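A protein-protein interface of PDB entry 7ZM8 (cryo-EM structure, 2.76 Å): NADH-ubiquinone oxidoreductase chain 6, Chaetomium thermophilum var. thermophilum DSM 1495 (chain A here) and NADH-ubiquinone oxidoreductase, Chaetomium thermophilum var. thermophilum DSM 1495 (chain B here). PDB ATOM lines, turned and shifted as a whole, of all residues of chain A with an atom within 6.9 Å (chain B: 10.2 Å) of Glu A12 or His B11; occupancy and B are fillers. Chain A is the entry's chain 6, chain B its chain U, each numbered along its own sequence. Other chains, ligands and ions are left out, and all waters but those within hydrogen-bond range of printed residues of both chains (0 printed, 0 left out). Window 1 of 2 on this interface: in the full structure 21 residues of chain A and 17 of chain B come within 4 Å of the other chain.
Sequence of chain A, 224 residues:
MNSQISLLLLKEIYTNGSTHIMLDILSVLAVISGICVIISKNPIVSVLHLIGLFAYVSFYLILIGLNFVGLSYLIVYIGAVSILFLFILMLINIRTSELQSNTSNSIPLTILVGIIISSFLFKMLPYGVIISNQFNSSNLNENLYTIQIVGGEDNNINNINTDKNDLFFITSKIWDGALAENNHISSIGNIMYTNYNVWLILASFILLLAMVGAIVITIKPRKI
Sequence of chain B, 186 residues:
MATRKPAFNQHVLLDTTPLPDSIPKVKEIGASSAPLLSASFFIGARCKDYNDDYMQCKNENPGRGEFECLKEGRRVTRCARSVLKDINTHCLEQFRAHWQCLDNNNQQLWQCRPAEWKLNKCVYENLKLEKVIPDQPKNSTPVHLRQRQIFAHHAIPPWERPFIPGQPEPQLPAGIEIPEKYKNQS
ND2 of Asn B9 lies within hydrogen-bond range of OE2 of Glu A12, 2.7 Å away.
The side-chain amide nitrogen (ND2) of Asn B9 is in hydrogen-bond range of the backbone carbonyl oxygen (O) of Thr A15 (3.0 Å).
O of Asn B9 sits close to O of Asn A16 (2.7 Å).
O of Gln B10 sits at hydrogen-bond distance from N of Glu A12, at 2.9 Å.
The backbone carbonyl oxygen (O) of Asn A16 sits at hydrogen-bond distance from the side-chain amide nitrogen (NE2) of Gln B10 (2.8 Å).
The backbone carbonyl oxygen (O) of Leu A10 sits close to a ring nitrogen (ND1) of His B11 (3.3 Å).
N of His B11 sits close to OE1 of Glu A12 (3.4 Å).
The backbone carbonyl oxygen (O) of Leu A10 sits at hydrogen-bond distance from the backbone NH (N) of Val B12 (2.8 Å).
The backbone carbonyl oxygen (O) of Ile A13 sits close to the side-chain amide oxygen (OD1) of Asn A16.
CA of Leu A9 touches O of Val B12, at 3.5 Å.
CA of Lys A11 touches O of Gln B10, 3.3 Å away.
Lys A11 touches His B11 (CA to ND1, 3.6 Å).
Glu A12 touches Val B12.
O of Ala B7 touches CA of Gly A17, at 3.8 Å.
Asn B9 touches Gly A17 (O to N, 3.6 Å).
NE2 of Gln B10 touches C of Gly A17 (3.9 Å).
Ile A170 touches Leu B13 (CD1 to CB, 3.99 Å).
Glu A12 touches four residues of chain B.
His B11 touches just these residues of chain A: Leu A10 (3.0 Å), Lys A11 (3.6 Å) and Glu A12 (2.8 Å).
Of the printed residues of chain B, Lys A11 touches Gln B10 (3.3 Å) and His B11 (3.6 Å).
Ile A13 touches none of the printed residues of chain B.
Of chain B, only Asn B9 (2.7 Å) and Gln B10 (2.8 Å) come within 4 Å of Asn A16.
Printed residues of chain A within 4 Å of Gln B10: Lys A11 (3.3 Å), Glu A12 (2.9 Å), Asn A16 (2.8 Å) and Gly A17 (3.9 Å).
Printed residues of chain B within 4 Å of Gly A17: Ala B7, Asn B9 and Gln B10.
The nearest printed residue of chain B that does not touch Glu A12 is Pro B6 (6.4 Å).
Of the 10 printed residues of chain B, 6 touch a printed residue of chain A.
Hydrophobic or aromatic side chains of chain B within 4 Å of the printed part of chain A: His B11, Val B12 and Leu B13.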
ATOM      1  N   LEU A   9       7.082 -14.656  14.193  1.00  0.00           N
ATOM      2  CA  LEU A   9       8.141 -14.041  15.040  1.00  0.00           C
ATOM      3  C   LEU A   9       9.086 -15.133  15.557  1.00  0.00           C
ATOM      4  O   LEU A   9       8.582 -16.108  16.123  1.00  0.00           O
ATOM      5  CB  LEU A   9       7.467 -13.278  16.183  1.00  0.00           C
ATOM      6  CG  LEU A   9       8.280 -12.137  16.790  1.00  0.00           C
ATOM      7  CD1 LEU A   9       8.741 -11.167  15.713  1.00  0.00           C
ATOM      8  CD2 LEU A   9       7.466 -11.408  17.845  1.00  0.00           C
ATOM      9  N   LEU A  10      10.398 -14.979  15.354  1.00  0.00           N
ATOM     10  CA  LEU A  10      11.395 -16.011  15.755  1.00  0.00           C
ATOM     11  C   LEU A  10      12.554 -15.342  16.498  1.00  0.00           C
ATOM     12  O   LEU A  10      12.753 -14.142  16.295  1.00  0.00           O
ATOM     13  CB  LEU A  10      11.960 -16.671  14.495  1.00  0.00           C
ATOM     14  CG  LEU A  10      11.098 -17.720  13.808  1.00  0.00           C
ATOM     15  CD1 LEU A  10      10.383 -17.115  12.609  1.00  0.00           C
ATOM     16  CD2 LEU A  10      11.973 -18.881  13.369  1.00  0.00           C
ATOM     17  N   LYS A  11      13.296 -16.093  17.313  1.00  0.00           N
ATOM     18  CA  LYS A  11      14.496 -15.532  17.988  1.00  0.00           C
ATOM     19  C   LYS A  11      15.722 -15.721  17.094  1.00  0.00           C
ATOM     20  O   LYS A  11      15.928 -16.848  16.628  1.00  0.00           O
ATOM     21  CB  LYS A  11      14.739 -16.208  19.338  1.00  0.00           C
ATOM     22  CG  LYS A  11      15.763 -15.522  20.229  1.00  0.00           C
ATOM     23  CD  LYS A  11      15.883 -16.148  21.600  1.00  0.00           C
ATOM     24  CE  LYS A  11      16.830 -15.396  22.511  1.00  0.00           C
ATOM     25  NZ  LYS A  11      16.886 -15.999  23.864  1.00  0.00           N
ATOM     26  N   GLU A  12      16.491 -14.651  16.851  1.00  0.00           N
ATOM     27  CA  GLU A  12      17.754 -14.766  16.076  1.00  0.00           C
ATOM     28  C   GLU A  12      18.770 -15.608  16.853  1.00  0.00           C
ATOM     29  O   GLU A  12      18.722 -15.584  18.093  1.00  0.00           O
ATOM     30  CB  GLU A  12      18.305 -13.378  15.771  1.00  0.00           C
ATOM     31  CG  GLU A  12      17.235 -12.402  15.339  1.00  0.00           C
ATOM     32  CD  GLU A  12      17.756 -10.997  15.115  1.00  0.00           C
ATOM     33  OE1 GLU A  12      16.937 -10.084  14.926  1.00  0.00           O
ATOM     34  OE2 GLU A  12      18.982 -10.829  15.126  1.00  0.00           O
ATOM     35  N   ILE A  13      19.684 -16.287  16.158  1.00  0.00           N
ATOM     36  CA  ILE A  13      20.608 -17.191  16.902  1.00  0.00           C
ATOM     37  C   ILE A  13      22.064 -16.694  16.942  1.00  0.00           C
ATOM     38  O   ILE A  13      22.627 -16.689  18.051  1.00  0.00           O
ATOM     39  CB  ILE A  13      20.428 -18.653  16.438  1.00  0.00           C
ATOM     40  CG1 ILE A  13      21.347 -19.615  17.192  1.00  0.00           C
ATOM     41  CG2 ILE A  13      20.572 -18.778  14.929  1.00  0.00           C
ATOM     42  CD1 ILE A  13      21.073 -21.073  16.908  1.00  0.00           C
ATOM     43  N   TYR A  14      22.673 -16.293  15.824  1.00  0.00           N
ATOM     44  CA  TYR A  14      24.118 -15.926  15.896  1.00  0.00           C
ATOM     45  C   TYR A  14      24.348 -14.451  15.567  1.00  0.00           C
ATOM     46  O   TYR A  14      25.480 -13.972  15.747  1.00  0.00           O
ATOM     47  CB  TYR A  14      24.961 -16.854  15.025  1.00  0.00           C
ATOM     48  CG  TYR A  14      24.990 -18.286  15.490  1.00  0.00           C
ATOM     49  CD1 TYR A  14      25.707 -18.657  16.615  1.00  0.00           C
ATOM     50  CD2 TYR A  14      24.306 -19.275  14.805  1.00  0.00           C
ATOM     51  CE1 TYR A  14      25.742 -19.969  17.052  1.00  0.00           C
ATOM     52  CE2 TYR A  14      24.331 -20.594  15.228  1.00  0.00           C
ATOM     53  CZ  TYR A  14      25.051 -20.943  16.354  1.00  0.00           C
ATOM     54  OH  TYR A  14      25.081 -22.242  16.772  1.00  0.00           O
ATOM     55  N   THR A  15      23.304 -13.753  15.123  1.00  0.00           N
ATOM     56  CA  THR A  15      23.389 -12.314  14.780  1.00  0.00           C
ATOM     57  C   THR A  15      22.402 -11.618  15.712  1.00  0.00           C
ATOM     58  O   THR A  15      21.747 -10.679  15.255  1.00  0.00           O
ATOM     59  CB  THR A  15      23.039 -12.149  13.300  1.00  0.00           C
ATOM     60  OG1 THR A  15      21.771 -12.773  13.096  1.00  0.00           O
ATOM     61  CG2 THR A  15      24.059 -12.786  12.381  1.00  0.00           C
ATOM     62  N   ASN A  16      22.358 -12.010  16.986  1.00  0.00           N
ATOM     63  CA  ASN A  16      21.293 -11.555  17.919  1.00  0.00           C
ATOM     64  C   ASN A  16      21.583 -10.243  18.651  1.00  0.00           C
ATOM     65  O   ASN A  16      20.967 -10.056  19.697  1.00  0.00           O
ATOM     66  CB  ASN A  16      20.940 -12.640  18.934  1.00  0.00           C
ATOM     67  CG  ASN A  16      22.155 -13.203  19.643  1.00  0.00           C
ATOM     68  OD1 ASN A  16      23.038 -13.779  19.012  1.00  0.00           O
ATOM     69  ND2 ASN A  16      22.198 -13.053  20.956  1.00  0.00           N
ATOM     70  N   GLY A  17      22.543  -9.428  18.230  1.00  0.00           N
ATOM     71  CA  GLY A  17      22.712  -8.089  18.843  1.00  0.00           C
ATOM     72  C   GLY A  17      22.841  -8.061  20.359  1.00  0.00           C
ATOM     73  O   GLY A  17      23.417  -9.013  20.915  1.00  0.00           O
ATOM     74  N   PHE A 168       7.483  -2.105  17.580  1.00  0.00           N
ATOM     75  CA  PHE A 168       8.834  -2.689  17.433  1.00  0.00           C
ATOM     76  C   PHE A 168       9.462  -1.968  16.243  1.00  0.00           C
ATOM     77  O   PHE A 168       8.723  -1.609  15.332  1.00  0.00           O
ATOM     78  CB  PHE A 168       8.753  -4.199  17.205  1.00  0.00           C
ATOM     79  CG  PHE A 168       8.670  -5.042  18.451  1.00  0.00           C
ATOM     80  CD1 PHE A 168       7.457  -5.264  19.082  1.00  0.00           C
ATOM     81  CD2 PHE A 168       9.803  -5.633  18.982  1.00  0.00           C
ATOM     82  CE1 PHE A 168       7.382  -6.045  20.223  1.00  0.00           C
ATOM     83  CE2 PHE A 168       9.728  -6.414  20.125  1.00  0.00           C
ATOM     84  CZ  PHE A 168       8.517  -6.619  20.742  1.00  0.00           C
ATOM     85  N   ILE A 170      11.448  -2.123  12.923  1.00  0.00           N
ATOM     86  CA  ILE A 170      11.821  -3.121  11.879  1.00  0.00           C
ATOM     87  C   ILE A 170      13.013  -2.611  11.065  1.00  0.00           C
ATOM     88  O   ILE A 170      13.086  -1.405  10.818  1.00  0.00           O
ATOM     89  CB  ILE A 170      10.610  -3.519  11.003  1.00  0.00           C
ATOM     90  CG1 ILE A 170      10.867  -4.794  10.198  1.00  0.00           C
ATOM     91  CG2 ILE A 170      10.135  -2.374  10.125  1.00  0.00           C
ATOM     92  CD1 ILE A 170      10.582  -6.060  10.960  1.00  0.00           C
ATOM     93  N   LYS B   5      21.560  -0.023  10.639  1.00  0.00           N
ATOM     94  CA  LYS B   5      22.103  -1.275  11.199  1.00  0.00           C
ATOM     95  C   LYS B   5      21.437  -1.478  12.564  1.00  0.00           C
ATOM     96  O   LYS B   5      21.361  -0.503  13.329  1.00  0.00           O
ATOM     97  CB  LYS B   5      23.606  -1.086  11.333  1.00  0.00           C
ATOM     98  CG  LYS B   5      24.355  -0.834  10.032  1.00  0.00           C
ATOM     99  CD  LYS B   5      25.711  -0.200  10.250  1.00  0.00           C
ATOM    100  CE  LYS B   5      26.721  -0.584   9.191  1.00  0.00           C
ATOM    101  NZ  LYS B   5      27.139  -1.999   9.331  1.00  0.00           N
ATOM    102  N   PRO B   6      20.959  -2.687  12.925  1.00  0.00           N
ATOM    103  CA  PRO B   6      20.369  -2.883  14.237  1.00  0.00           C
ATOM    104  C   PRO B   6      21.356  -3.080  15.406  1.00  0.00           C
ATOM    105  O   PRO B   6      22.374  -3.698  15.208  1.00  0.00           O
ATOM    106  CB  PRO B   6      19.475  -4.089  13.954  1.00  0.00           C
ATOM    107  CG  PRO B   6      20.239  -4.902  12.944  1.00  0.00           C
ATOM    108  CD  PRO B   6      20.934  -3.877  12.078  1.00  0.00           C
ATOM    109  N   ALA B   7      21.012  -2.584  16.602  1.00  0.00           N
ATOM    110  CA  ALA B   7      21.896  -2.716  17.745  1.00  0.00           C
ATOM    111  C   ALA B   7      21.411  -3.703  18.794  1.00  0.00           C
ATOM    112  O   ALA B   7      22.245  -4.330  19.451  1.00  0.00           O
ATOM    113  CB  ALA B   7      22.106  -1.349  18.419  1.00  0.00           C
ATOM    114  N   PHE B   8      20.095  -3.839  18.941  1.00  0.00           N
ATOM    115  CA  PHE B   8      19.517  -4.714  19.989  1.00  0.00           C
ATOM    116  C   PHE B   8      18.473  -5.639  19.357  1.00  0.00           C
ATOM    117  O   PHE B   8      17.384  -5.783  19.925  1.00  0.00           O
ATOM    118  CB  PHE B   8      18.925  -3.859  21.111  1.00  0.00           C
ATOM    119  CG  PHE B   8      19.830  -2.767  21.615  1.00  0.00           C
ATOM    120  CD1 PHE B   8      20.934  -3.062  22.392  1.00  0.00           C
ATOM    121  CD2 PHE B   8      19.575  -1.442  21.306  1.00  0.00           C
ATOM    122  CE1 PHE B   8      21.771  -2.055  22.843  1.00  0.00           C
ATOM    123  CE2 PHE B   8      20.412  -0.436  21.756  1.00  0.00           C
ATOM    124  CZ  PHE B   8      21.509  -0.746  22.521  1.00  0.00           C
ATOM    125  N   ASN B   9      18.788  -6.233  18.208  1.00  0.00           N
ATOM    126  CA  ASN B   9      17.841  -7.132  17.498  1.00  0.00           C
ATOM    127  C   ASN B   9      17.874  -8.517  18.146  1.00  0.00           C
ATOM    128  O   ASN B   9      18.950  -9.093  18.203  1.00  0.00           O
ATOM    129  CB  ASN B   9      18.191  -7.238  16.012  1.00  0.00           C
ATOM    130  CG  ASN B   9      19.673  -7.383  15.731  1.00  0.00           C
ATOM    131  OD1 ASN B   9      20.499  -6.656  16.278  1.00  0.00           O
ATOM    132  ND2 ASN B   9      20.025  -8.304  14.851  1.00  0.00           N
ATOM    133  N   GLN B  10      16.731  -9.029  18.603  1.00  0.00           N
ATOM    134  CA  GLN B  10      16.693 -10.404  19.163  1.00  0.00           C
ATOM    135  C   GLN B  10      15.695 -11.268  18.395  1.00  0.00           C
ATOM    136  O   GLN B  10      15.739 -12.490  18.571  1.00  0.00           O
ATOM    137  CB  GLN B  10      16.308 -10.353  20.645  1.00  0.00           C
ATOM    138  CG  GLN B  10      17.257  -9.528  21.503  1.00  0.00           C
ATOM    139  CD  GLN B  10      18.587 -10.209  21.705  1.00  0.00           C
ATOM    140  OE1 GLN B  10      18.709 -11.427  21.608  1.00  0.00           O
ATOM    141  NE2 GLN B  10      19.603  -9.418  22.001  1.00  0.00           N
ATOM    142  N   HIS B  11      14.847 -10.658  17.566  1.00  0.00           N
ATOM    143  CA  HIS B  11      13.768 -11.418  16.881  1.00  0.00           C
ATOM    144  C   HIS B  11      13.713 -11.089  15.389  1.00  0.00           C
ATOM    145  O   HIS B  11      14.097  -9.976  15.017  1.00  0.00           O
ATOM    146  CB  HIS B  11      12.417 -11.158  17.566  1.00  0.00           C
ATOM    147  CG  HIS B  11      12.359 -11.605  18.986  1.00  0.00           C
ATOM    148  ND1 HIS B  11      12.335 -12.939  19.336  1.00  0.00           N
ATOM    149  CD2 HIS B  11      12.314 -10.909  20.140  1.00  0.00           C
ATOM    150  CE1 HIS B  11      12.283 -13.046  20.646  1.00  0.00           C
ATOM    151  NE2 HIS B  11      12.269 -11.815  21.162  1.00  0.00           N
ATOM    152  N   VAL B  12      13.233 -12.033  14.577  1.00  0.00           N
ATOM    153  CA  VAL B  12      13.110 -11.835  13.105  1.00  0.00           C
ATOM    154  C   VAL B  12      11.626 -11.912  12.745  1.00  0.00           C
ATOM    155  O   VAL B  12      10.946 -12.800  13.278  1.00  0.00           O
ATOM    156  CB  VAL B  12      13.935 -12.882  12.332  1.00  0.00           C
ATOM    157  CG1 VAL B  12      13.401 -13.120  10.931  1.00  0.00           C
ATOM    158  CG2 VAL B  12      15.411 -12.525  12.293  1.00  0.00           C
ATOM    159  N   LEU B  13      11.141 -10.982  11.924  1.00  0.00           N
ATOM    160  CA  LEU B  13       9.734 -11.053  11.457  1.00  0.00           C
ATOM    161  C   LEU B  13       9.705 -11.539  10.010  1.00  0.00           C
ATOM    162  O   LEU B  13      10.253 -10.841   9.150  1.00  0.00           O
ATOM    163  CB  LEU B  13       9.055  -9.690  11.603  1.00  0.00           C
ATOM    164  CG  LEU B  13       7.570  -9.650  11.256  1.00  0.00           C
ATOM    165  CD1 LEU B  13       6.778 -10.603  12.134  1.00  0.00           C
ATOM    166  CD2 LEU B  13       7.029  -8.237  11.384  1.00  0.00           C
ATOM    167  N   LEU B  14       9.115 -12.708   9.774  1.00  0.00           N
ATOM    168  CA  LEU B  14       8.964 -13.226   8.398  1.00  0.00           C
ATOM    169  C   LEU B  14       7.534 -12.971   7.942  1.00  0.00           C
ATOM    170  O   LEU B  14       6.684 -12.681   8.797  1.00  0.00           O
ATOM    171  CB  LEU B  14       9.294 -14.719   8.360  1.00  0.00           C
ATOM    172  CG  LEU B  14      10.750 -15.086   8.641  1.00  0.00           C
ATOM    173  CD1 LEU B  14      10.963 -16.582   8.493  1.00  0.00           C
ATOM    174  CD2 LEU B  14      11.685 -14.330   7.714  1.00  0.00           C
